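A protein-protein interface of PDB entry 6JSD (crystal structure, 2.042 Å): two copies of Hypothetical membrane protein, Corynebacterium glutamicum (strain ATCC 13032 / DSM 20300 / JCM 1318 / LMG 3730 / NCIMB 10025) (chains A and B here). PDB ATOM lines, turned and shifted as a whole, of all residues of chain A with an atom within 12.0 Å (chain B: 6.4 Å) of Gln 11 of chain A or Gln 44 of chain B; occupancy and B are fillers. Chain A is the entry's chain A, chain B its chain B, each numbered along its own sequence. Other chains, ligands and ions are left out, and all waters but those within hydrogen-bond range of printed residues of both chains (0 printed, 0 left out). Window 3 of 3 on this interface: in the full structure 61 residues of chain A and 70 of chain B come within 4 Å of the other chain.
The backbone NH of Gln 11 of chain A sits at hydrogen-bond distance from the backbone carbonyl oxygen of Ser 160 of chain B. The side-chain amide oxygen (OE1) of Gln 11 of chain A is in hydrogen-bond range of the side-chain amide nitrogen (NE2) of Gln 44 of chain B (2.9 Å). The backbone NH (N) of Phe 45 of chain B sits at hydrogen-bond distance from the backbone carbonyl oxygen (O) of Ala 10 of chain A (3.0 Å). The backbone carbonyl oxygen of Pro 158 of chain B lies within hydrogen-bond range of the backbone NH of Gly 13 of chain A (3.0 Å). The side-chain amide oxygen of Gln 11 of chain A is in hydrogen-bond range of the side-chain amide nitrogen of Gln 42 of chain B. The backbone carbonyl oxygen (O) of Trp 12 of chain A sits at hydrogen-bond distance from the backbone NH (N) of Phe 43 of chain B.
OE1 of Gln 42 of chain B sits close to O of Pro 158 of chain B (3.4 Å). The backbone carbonyl oxygen (O) of Gln 42 of chain B lies within hydrogen-bond range of the side-chain amide nitrogen (NE2) of Gln 44 of chain B (3.1 Å). The backbone NH (N) of Gln 44 of chain B lies within hydrogen-bond range of the backbone carbonyl oxygen (O) of Gly 37 of chain B, at 2.8 Å. The side-chain amide nitrogen (NE2) of Gln 44 of chain B sits at hydrogen-bond distance from the backbone carbonyl oxygen (O) of Asp 39 of chain B, at 3.0 Å.
Ser 46 of chain B touches Ala 8 of chain A (CA to O, 3.5 Å). Phe 161 of chain B touches Ser 9 of chain A. O of Phe 43 of chain B touches O of Ala 10 of chain A (3.9 Å). Ala 10 of chain A touches Gln 44 of chain B. Ala 10 of chain A touches Ile 85 of chain B (CB to CD1, 3.97 Å). Gln 11 of chain A touches Pro 158 of chain B (O to O, 3.9 Å). O of Trp 12 of chain A touches CA of Gln 42 of chain B, at 3.7 Å. Trp 12 of chain A touches Pro 158 of chain B. Val 14 of chain A touches Phe 43 of chain B (CG2 to CD2, 3.5 Å). NZ of Lys 15 of chain A touches CZ of Phe 38 of chain B, at 3.8 Å.
Gln 11 of chain A touches just these residues of chain B: Gln 42, Phe 43, Gln 44, Pro 158, Ile 159 and Ser 160. No residue of chain A comes within 4 Å of Gly 35 of chain B. No residue of chain A comes within 4 Å of Val 36 of chain B. Of the printed residues of chain A, Phe 38 of chain B touches Lys 15 (3.8 Å). No residue of chain A comes within 4 Å of Asp 39 of chain B. Printed residues of chain A within 4 Å of Gln 42 of chain B: Gln 11, Trp 12 and Gly 13. Of chain A, only Ala 10, Gln 11, Trp 12, Gly 13 and Val 14 come within 4 Å of Phe 43 of chain B. Of chain A, only Ala 8 (3.5 Å) comes within 4 Å of Ser 46 of chain B. Pro 158 of chain B touches just these residues of chain A: Gln 11, Trp 12 and Gly 13. Of chain A, only Ala 10 (3.1 Å) and Gln 11 (2.8 Å) come within 4 Å of Ser 160 of chain B. Printed residues of chain A within 4 Å of Ile 159 of chain B: Gln 11 and Trp 12. Of the printed residues of chain A, Phe 45 of chain B touches Ser 9 (3.3 Å) and Ala 10 (3.0 Å). Of the printed residues of chain B, Trp 12 of chain A touches Gln 42, Phe 43, Pro 158 and Ile 159. Of the printed residues of chain B, Ser 9 of chain A touches Phe 45 and Phe 161. Gln 7 of chain A touches none of the printed residues of chain B. The nearest residue of chain A that does not touch Gln 44 of chain B is Trp 12 of chain A (5.2 Å). The nearest printed residue of chain B that does not touch Ala 10 of chain A is Phe 161 of chain B (4.1 Å).
Of the 17 printed residues of chain B, 11 touch a printed residue of chain A. Printed residues of chain B that touch a printed residue of chain A: Phe 38, Gln 42, Phe 43, Gln 44, Phe 45, Ser 46, Ile 85, Pro 158, Ile 159, Ser 160 and Phe 161. Of the 11 printed residues of chain A, 8 touch a printed residue of chain B. Hydrophobic or aromatic side chains of chain A within 4 Å of the printed part of chain B: Ala 10, Trp 12 and Val 14. Among the printed residues, 23 pairs touch across the chains. Among the printed residues, no Asp or Glu carboxylate lies within 4 Å of a Lys or Arg side-chain nitrogen of the other chain.
No position is printed for both chains. Of the 23 pairs that touch across the chains among the printed residues, none has its exchanged pair printed and touching as well.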
ATOM      1  N   GLN A   7      12.072  25.087   9.269  1.00  0.00           N
ATOM      2  CA  GLN A   7      12.641  25.408   7.973  1.00  0.00           C
ATOM      3  C   GLN A   7      11.993  24.497   6.945  1.00  0.00           C
ATOM      4  O   GLN A   7      11.328  23.517   7.287  1.00  0.00           O
ATOM      5  CB  GLN A   7      14.167  25.286   7.957  1.00  0.00           C
ATOM      6  CG  GLN A   7      14.700  23.915   8.281  1.00  0.00           C
ATOM      7  CD  GLN A   7      16.164  23.776   7.921  1.00  0.00           C
ATOM      8  OE1 GLN A   7      16.666  24.472   7.033  1.00  0.00           O
ATOM      9  NE2 GLN A   7      16.860  22.875   8.611  1.00  0.00           N
ATOM     10  N   ALA A   8      12.176  24.847   5.677  1.00  0.00           N
ATOM     11  CA  ALA A   8      11.499  24.137   4.603  1.00  0.00           C
ATOM     12  C   ALA A   8      12.245  24.342   3.294  1.00  0.00           C
ATOM     13  O   ALA A   8      12.973  25.317   3.110  1.00  0.00           O
ATOM     14  CB  ALA A   8      10.046  24.595   4.462  1.00  0.00           C
ATOM     15  N   SER A   9      12.052  23.388   2.388  1.00  0.00           N
ATOM     16  CA  SER A   9      12.602  23.454   1.043  1.00  0.00           C
ATOM     17  C   SER A   9      11.516  23.064   0.056  1.00  0.00           C
ATOM     18  O   SER A   9      10.590  22.320   0.389  1.00  0.00           O
ATOM     19  CB  SER A   9      13.804  22.521   0.838  1.00  0.00           C
ATOM     20  OG  SER A   9      14.863  22.808   1.724  1.00  0.00           O
ATOM     21  N   ALA A  10      11.633  23.574  -1.155  1.00  0.00           N
ATOM     22  CA  ALA A  10      10.710  23.198  -2.204  1.00  0.00           C
ATOM     23  C   ALA A  10      11.460  23.150  -3.519  1.00  0.00           C
ATOM     24  O   ALA A  10      12.502  23.788  -3.689  1.00  0.00           O
ATOM     25  CB  ALA A  10       9.532  24.179  -2.295  1.00  0.00           C
ATOM     26  N   GLN A  11      10.892  22.398  -4.456  1.00  0.00           N
ATOM     27  CA  GLN A  11      11.399  22.269  -5.810  1.00  0.00           C
ATOM     28  C   GLN A  11      10.224  22.376  -6.762  1.00  0.00           C
ATOM     29  O   GLN A  11       9.191  21.745  -6.547  1.00  0.00           O
ATOM     30  CB  GLN A  11      12.092  20.903  -6.043  1.00  0.00           C
ATOM     31  CG  GLN A  11      13.291  20.618  -5.197  1.00  0.00           C
ATOM     32  CD  GLN A  11      14.024  19.370  -5.711  1.00  0.00           C
ATOM     33  OE1 GLN A  11      14.650  19.396  -6.776  1.00  0.00           O
ATOM     34  NE2 GLN A  11      13.909  18.272  -4.978  1.00  0.00           N
ATOM     35  N   TRP A  12      10.395  23.136  -7.835  1.00  0.00           N
ATOM     36  CA  TRP A  12       9.297  23.352  -8.765  1.00  0.00           C
ATOM     37  C   TRP A  12       9.879  23.566 -10.156  1.00  0.00           C
ATOM     38  O   TRP A  12      10.779  24.393 -10.327  1.00  0.00           O
ATOM     39  CB  TRP A  12       8.454  24.560  -8.301  1.00  0.00           C
ATOM     40  CG  TRP A  12       7.384  24.932  -9.240  1.00  0.00           C
ATOM     41  CD1 TRP A  12       6.732  24.112 -10.127  1.00  0.00           C
ATOM     42  CD2 TRP A  12       6.852  26.239  -9.434  1.00  0.00           C
ATOM     43  NE1 TRP A  12       5.811  24.836 -10.844  1.00  0.00           N
ATOM     44  CE2 TRP A  12       5.876  26.147 -10.448  1.00  0.00           C
ATOM     45  CE3 TRP A  12       7.103  27.481  -8.842  1.00  0.00           C
ATOM     46  CZ2 TRP A  12       5.156  27.251 -10.886  1.00  0.00           C
ATOM     47  CZ3 TRP A  12       6.393  28.581  -9.288  1.00  0.00           C
ATOM     48  CH2 TRP A  12       5.422  28.458 -10.295  1.00  0.00           C
ATOM     49  N   GLY A  13       9.382  22.809 -11.140  1.00  0.00           N
ATOM     50  CA  GLY A  13       9.974  22.861 -12.469  1.00  0.00           C
ATOM     51  C   GLY A  13       9.822  24.215 -13.140  1.00  0.00           C
ATOM     52  O   GLY A  13      10.751  24.700 -13.792  1.00  0.00           O
ATOM     53  N   VAL A  14       8.643  24.828 -13.011  1.00  0.00           N
ATOM     54  CA  VAL A  14       8.265  26.101 -13.635  1.00  0.00           C
ATOM     55  C   VAL A  14       8.265  26.034 -15.167  1.00  0.00           C
ATOM     56  O   VAL A  14       7.271  26.404 -15.801  1.00  0.00           O
ATOM     57  CB  VAL A  14       9.148  27.270 -13.161  1.00  0.00           C
ATOM     58  CG1 VAL A  14       8.640  28.543 -13.783  1.00  0.00           C
ATOM     59  CG2 VAL A  14       9.120  27.391 -11.633  1.00  0.00           C
ATOM     60  N   LYS A  15       9.366  25.568 -15.770  1.00  0.00           N
ATOM     61  CA  LYS A  15       9.508  25.616 -17.230  1.00  0.00           C
ATOM     62  C   LYS A  15       8.415  24.822 -17.952  1.00  0.00           C
ATOM     63  O   LYS A  15       7.930  25.248 -19.009  1.00  0.00           O
ATOM     64  CB  LYS A  15      10.892  25.102 -17.648  1.00  0.00           C
ATOM     65  CG  LYS A  15      12.041  26.027 -17.267  1.00  0.00           C
ATOM     66  CD  LYS A  15      13.338  25.622 -17.963  1.00  0.00           C
ATOM     67  CE  LYS A  15      14.523  26.323 -17.307  1.00  0.00           C
ATOM     68  NZ  LYS A  15      15.837  25.793 -17.792  1.00  0.00           N
ATOM     69  N   ALA A  16       8.033  23.657 -17.421  1.00  0.00           N
ATOM     70  CA  ALA A  16       6.930  22.902 -18.024  1.00  0.00           C
ATOM     71  C   ALA A  16       5.639  23.723 -18.074  1.00  0.00           C
ATOM     72  O   ALA A  16       4.896  23.662 -19.061  1.00  0.00           O
ATOM     73  CB  ALA A  16       6.683  21.612 -17.252  1.00  0.00           C
ATOM     74  N   SER A  17       5.337  24.472 -17.004  1.00  0.00           N
ATOM     75  CA  SER A  17       4.113  25.272 -16.995  1.00  0.00           C
ATOM     76  C   SER A  17       4.182  26.403 -18.020  1.00  0.00           C
ATOM     77  O   SER A  17       3.163  26.747 -18.634  1.00  0.00           O
ATOM     78  CB  SER A  17       3.834  25.824 -15.589  1.00  0.00           C
ATOM     79  OG  SER A  17       3.320  24.799 -14.738  1.00  0.00           O
ATOM     80  N   GLY B  35      17.045  35.086  -4.842  1.00  0.00           N
ATOM     81  CA  GLY B  35      16.635  34.301  -3.689  1.00  0.00           C
ATOM     82  C   GLY B  35      16.106  32.929  -4.031  1.00  0.00           C
ATOM     83  O   GLY B  35      15.392  32.320  -3.216  1.00  0.00           O
ATOM     84  N   VAL B  36      16.419  32.434  -5.233  1.00  0.00           N
ATOM     85  CA  VAL B  36      15.938  31.160  -5.760  1.00  0.00           C
ATOM     86  C   VAL B  36      17.089  30.471  -6.492  1.00  0.00           C
ATOM     87  O   VAL B  36      17.872  31.128  -7.184  1.00  0.00           O
ATOM     88  CB  VAL B  36      14.750  31.356  -6.734  1.00  0.00           C
ATOM     89  CG1 VAL B  36      14.231  30.039  -7.193  1.00  0.00           C
ATOM     90  CG2 VAL B  36      13.631  32.176  -6.094  1.00  0.00           C
ATOM     91  N   GLY B  37      17.181  29.145  -6.366  1.00  0.00           N
ATOM     92  CA  GLY B  37      18.200  28.374  -7.044  1.00  0.00           C
ATOM     93  C   GLY B  37      17.631  27.565  -8.203  1.00  0.00           C
ATOM     94  O   GLY B  37      16.448  27.619  -8.519  1.00  0.00           O
ATOM     95  N   PHE B  38      18.510  26.770  -8.816  1.00  0.00           N
ATOM     96  CA  PHE B  38      18.103  25.881  -9.898  1.00  0.00           C
ATOM     97  C   PHE B  38      19.027  24.671  -9.931  1.00  0.00           C
ATOM     98  O   PHE B  38      20.251  24.822 -10.007  1.00  0.00           O
ATOM     99  CB  PHE B  38      18.119  26.590 -11.249  1.00  0.00           C
ATOM    100  CG  PHE B  38      17.378  25.849 -12.318  1.00  0.00           C
ATOM    101  CD1 PHE B  38      18.033  24.908 -13.115  1.00  0.00           C
ATOM    102  CD2 PHE B  38      16.029  26.075 -12.530  1.00  0.00           C
ATOM    103  CE1 PHE B  38      17.355  24.219 -14.094  1.00  0.00           C
ATOM    104  CE2 PHE B  38      15.348  25.379 -13.508  1.00  0.00           C
ATOM    105  CZ  PHE B  38      16.011  24.458 -14.290  1.00  0.00           C
ATOM    106  N   ASP B  39      18.433  23.481  -9.869  1.00  0.00           N
ATOM    107  CA  ASP B  39      19.172  22.227  -9.895  1.00  0.00           C
ATOM    108  C   ASP B  39      18.234  21.097 -10.287  1.00  0.00           C
ATOM    109  O   ASP B  39      17.039  21.147  -9.994  1.00  0.00           O
ATOM    110  CB  ASP B  39      19.788  21.919  -8.537  1.00  0.00           C
ATOM    111  CG  ASP B  39      20.645  20.675  -8.571  1.00  0.00           C
ATOM    112  OD1 ASP B  39      21.710  20.744  -9.214  1.00  0.00           O
ATOM    113  OD2 ASP B  39      20.248  19.643  -7.976  1.00  0.00           O
ATOM    114  N   ASN B  40      18.784  20.059 -10.934  1.00  0.00           N
ATOM    115  CA  ASN B  40      17.966  18.901 -11.265  1.00  0.00           C
ATOM    116  C   ASN B  40      16.725  19.338 -12.046  1.00  0.00           C
ATOM    117  O   ASN B  40      15.606  18.880 -11.791  1.00  0.00           O
ATOM    118  CB  ASN B  40      17.585  18.134  -9.991  1.00  0.00           C
ATOM    119  CG  ASN B  40      16.889  16.812 -10.276  1.00  0.00           C
ATOM    120  OD1 ASN B  40      17.174  16.136 -11.275  1.00  0.00           O
ATOM    121  ND2 ASN B  40      15.952  16.448  -9.405  1.00  0.00           N
ATOM    122  N   GLN B  41      16.924  20.298 -12.948  1.00  0.00           N
ATOM    123  CA  GLN B  41      15.872  20.837 -13.814  1.00  0.00           C
ATOM    124  C   GLN B  41      14.700  21.434 -13.040  1.00  0.00           C
ATOM    125  O   GLN B  41      13.576  21.474 -13.541  1.00  0.00           O
ATOM    126  CB  GLN B  41      15.376  19.764 -14.777  1.00  0.00           C
ATOM    127  CG  GLN B  41      16.489  19.175 -15.601  1.00  0.00           C
ATOM    128  CD  GLN B  41      16.058  17.906 -16.281  1.00  0.00           C
ATOM    129  OE1 GLN B  41      14.935  17.812 -16.767  1.00  0.00           O
ATOM    130  NE2 GLN B  41      16.935  16.907 -16.293  1.00  0.00           N
ATOM    131  N   GLN B  42      14.932  21.914 -11.820  1.00  0.00           N
ATOM    132  CA  GLN B  42      13.864  22.534 -11.045  1.00  0.00           C
ATOM    133  C   GLN B  42      14.395  23.741 -10.293  1.00  0.00           C
ATOM    134  O   GLN B  42      15.532  23.732  -9.810  1.00  0.00           O
ATOM    135  CB  GLN B  42      13.238  21.542 -10.046  1.00  0.00           C
ATOM    136  CG  GLN B  42      12.589  20.327 -10.693  1.00  0.00           C
ATOM    137  CD  GLN B  42      11.861  19.451  -9.704  1.00  0.00           C
ATOM    138  OE1 GLN B  42      10.722  19.731  -9.316  1.00  0.00           O
ATOM    139  NE2 GLN B  42      12.515  18.387  -9.283  1.00  0.00           N
ATOM    140  N   PHE B  43      13.567  24.779 -10.189  1.00  0.00           N
ATOM    141  CA  PHE B  43      13.906  25.891  -9.320  1.00  0.00           C
ATOM    142  C   PHE B  43      13.812  25.444  -7.869  1.00  0.00           C
ATOM    143  O   PHE B  43      13.001  24.587  -7.514  1.00  0.00           O
ATOM    144  CB  PHE B  43      12.981  27.098  -9.571  1.00  0.00           C
ATOM    145  CG  PHE B  43      13.227  27.756 -10.886  1.00  0.00           C
ATOM    146  CD1 PHE B  43      14.173  28.747 -11.006  1.00  0.00           C
ATOM    147  CD2 PHE B  43      12.559  27.322 -12.027  1.00  0.00           C
ATOM    148  CE1 PHE B  43      14.434  29.328 -12.233  1.00  0.00           C
ATOM    149  CE2 PHE B  43      12.802  27.902 -13.248  1.00  0.00           C
ATOM    150  CZ  PHE B  43      13.741  28.908 -13.358  1.00  0.00           C
ATOM    151  N   GLN B  44      14.652  26.050  -7.032  1.00  0.00           N
ATOM    152  CA  GLN B  44      14.927  25.589  -5.676  1.00  0.00           C
ATOM    153  C   GLN B  44      14.625  26.726  -4.704  1.00  0.00           C
ATOM    154  O   GLN B  44      15.136  27.830  -4.885  1.00  0.00           O
ATOM    155  CB  GLN B  44      16.394  25.186  -5.551  1.00  0.00           C
ATOM    156  CG  GLN B  44      16.840  24.132  -6.600  1.00  0.00           C
ATOM    157  CD  GLN B  44      16.294  22.748  -6.271  1.00  0.00           C
ATOM    158  OE1 GLN B  44      16.173  22.390  -5.101  1.00  0.00           O
ATOM    159  NE2 GLN B  44      15.936  21.974  -7.302  1.00  0.00           N
ATOM    160  N   PHE B  45      13.854  26.438  -3.660  1.00  0.00           N
ATOM    161  CA  PHE B  45      13.379  27.430  -2.705  1.00  0.00           C
ATOM    162  C   PHE B  45      13.757  27.009  -1.293  1.00  0.00           C
ATOM    163  O   PHE B  45      13.816  25.813  -0.988  1.00  0.00           O
ATOM    164  CB  PHE B  45      11.846  27.593  -2.789  1.00  0.00           C
ATOM    165  CG  PHE B  45      11.344  27.948  -4.160  1.00  0.00           C
ATOM    166  CD1 PHE B  45      11.217  26.969  -5.151  1.00  0.00           C
ATOM    167  CD2 PHE B  45      11.018  29.273  -4.472  1.00  0.00           C
ATOM    168  CE1 PHE B  45      10.755  27.299  -6.434  1.00  0.00           C
ATOM    169  CE2 PHE B  45      10.554  29.616  -5.739  1.00  0.00           C
ATOM    170  CZ  PHE B  45      10.429  28.636  -6.726  1.00  0.00           C
ATOM    171  N   SER B  46      14.005  28.003  -0.433  1.00  0.00           N
ATOM    172  CA  SER B  46      14.291  27.803   0.984  1.00  0.00           C
ATOM    173  C   SER B  46      13.470  28.810   1.775  1.00  0.00           C
ATOM    174  O   SER B  46      13.437  29.999   1.433  1.00  0.00           O
ATOM    175  CB  SER B  46      15.776  27.989   1.328  1.00  0.00           C
ATOM    176  OG  SER B  46      16.607  27.147   0.570  1.00  0.00           O
ATOM    177  N   ILE B  85       2.844  27.125  -1.002  1.00  0.00           N
ATOM    178  CA  ILE B  85       2.263  25.816  -1.270  1.00  0.00           C
ATOM    179  C   ILE B  85       1.170  25.565  -0.241  1.00  0.00           C
ATOM    180  O   ILE B  85       1.447  25.414   0.957  1.00  0.00           O
ATOM    181  CB  ILE B  85       3.314  24.701  -1.230  1.00  0.00           C
ATOM    182  CG1 ILE B  85       4.423  24.953  -2.269  1.00  0.00           C
ATOM    183  CG2 ILE B  85       2.624  23.353  -1.440  1.00  0.00           C
ATOM    184  CD1 ILE B  85       5.570  23.969  -2.185  1.00  0.00           C
ATOM    185  N   PRO B 158       6.563  19.305 -12.104  1.00  0.00           N
ATOM    186  CA  PRO B 158       6.534  18.734 -10.757  1.00  0.00           C
ATOM    187  C   PRO B 158       6.795  19.798  -9.707  1.00  0.00           C
ATOM    188  O   PRO B 158       7.498  20.778  -9.949  1.00  0.00           O
ATOM    189  CB  PRO B 158       7.672  17.706 -10.790  1.00  0.00           C
ATOM    190  CG  PRO B 158       8.690  18.345 -11.711  1.00  0.00           C
ATOM    191  CD  PRO B 158       7.890  19.151 -12.735  1.00  0.00           C
ATOM    192  N   ILE B 159       6.230  19.578  -8.529  1.00  0.00           N
ATOM    193  CA  ILE B 159       6.536  20.387  -7.354  1.00  0.00           C
ATOM    194  C   ILE B 159       6.588  19.472  -6.138  1.00  0.00           C
ATOM    195  O   ILE B 159       5.834  18.499  -6.045  1.00  0.00           O
ATOM    196  CB  ILE B 159       5.514  21.524  -7.151  1.00  0.00           C
ATOM    197  CG1 ILE B 159       5.937  22.432  -5.993  1.00  0.00           C
ATOM    198  CG2 ILE B 159       4.128  20.962  -6.913  1.00  0.00           C
ATOM    199  CD1 ILE B 159       5.262  23.822  -6.037  1.00  0.00           C
ATOM    200  N   SER B 160       7.500  19.770  -5.217  1.00  0.00           N
ATOM    201  CA  SER B 160       7.648  18.967  -4.016  1.00  0.00           C
ATOM    202  C   SER B 160       8.217  19.854  -2.922  1.00  0.00           C
ATOM    203  O   SER B 160       8.875  20.856  -3.205  1.00  0.00           O
ATOM    204  CB  SER B 160       8.578  17.771  -4.253  1.00  0.00           C
ATOM    205  OG  SER B 160       9.883  18.237  -4.536  1.00  0.00           O
ATOM    206  N   PHE B 161       7.998  19.444  -1.674  1.00  0.00           N
ATOM    207  CA  PHE B 161       8.495  20.191  -0.531  1.00  0.00           C
ATOM    208  C   PHE B 161       8.751  19.256   0.637  1.00  0.00           C
ATOM    209  O   PHE B 161       8.109  18.215   0.775  1.00  0.00           O
ATOM    210  CB  PHE B 161       7.501  21.277  -0.088  1.00  0.00           C
ATOM    211  CG  PHE B 161       6.266  20.734   0.596  1.00  0.00           C
ATOM    212  CD1 PHE B 161       5.173  20.327  -0.149  1.00  0.00           C
ATOM    213  CD2 PHE B 161       6.202  20.640   1.980  1.00  0.00           C
ATOM    214  CE1 PHE B 161       4.039  19.836   0.460  1.00  0.00           C
ATOM    215  CE2 PHE B 161       5.063  20.142   2.608  1.00  0.00           C
ATOM    216  CZ  PHE B 161       3.979  19.742   1.844  1.00  0.00           C
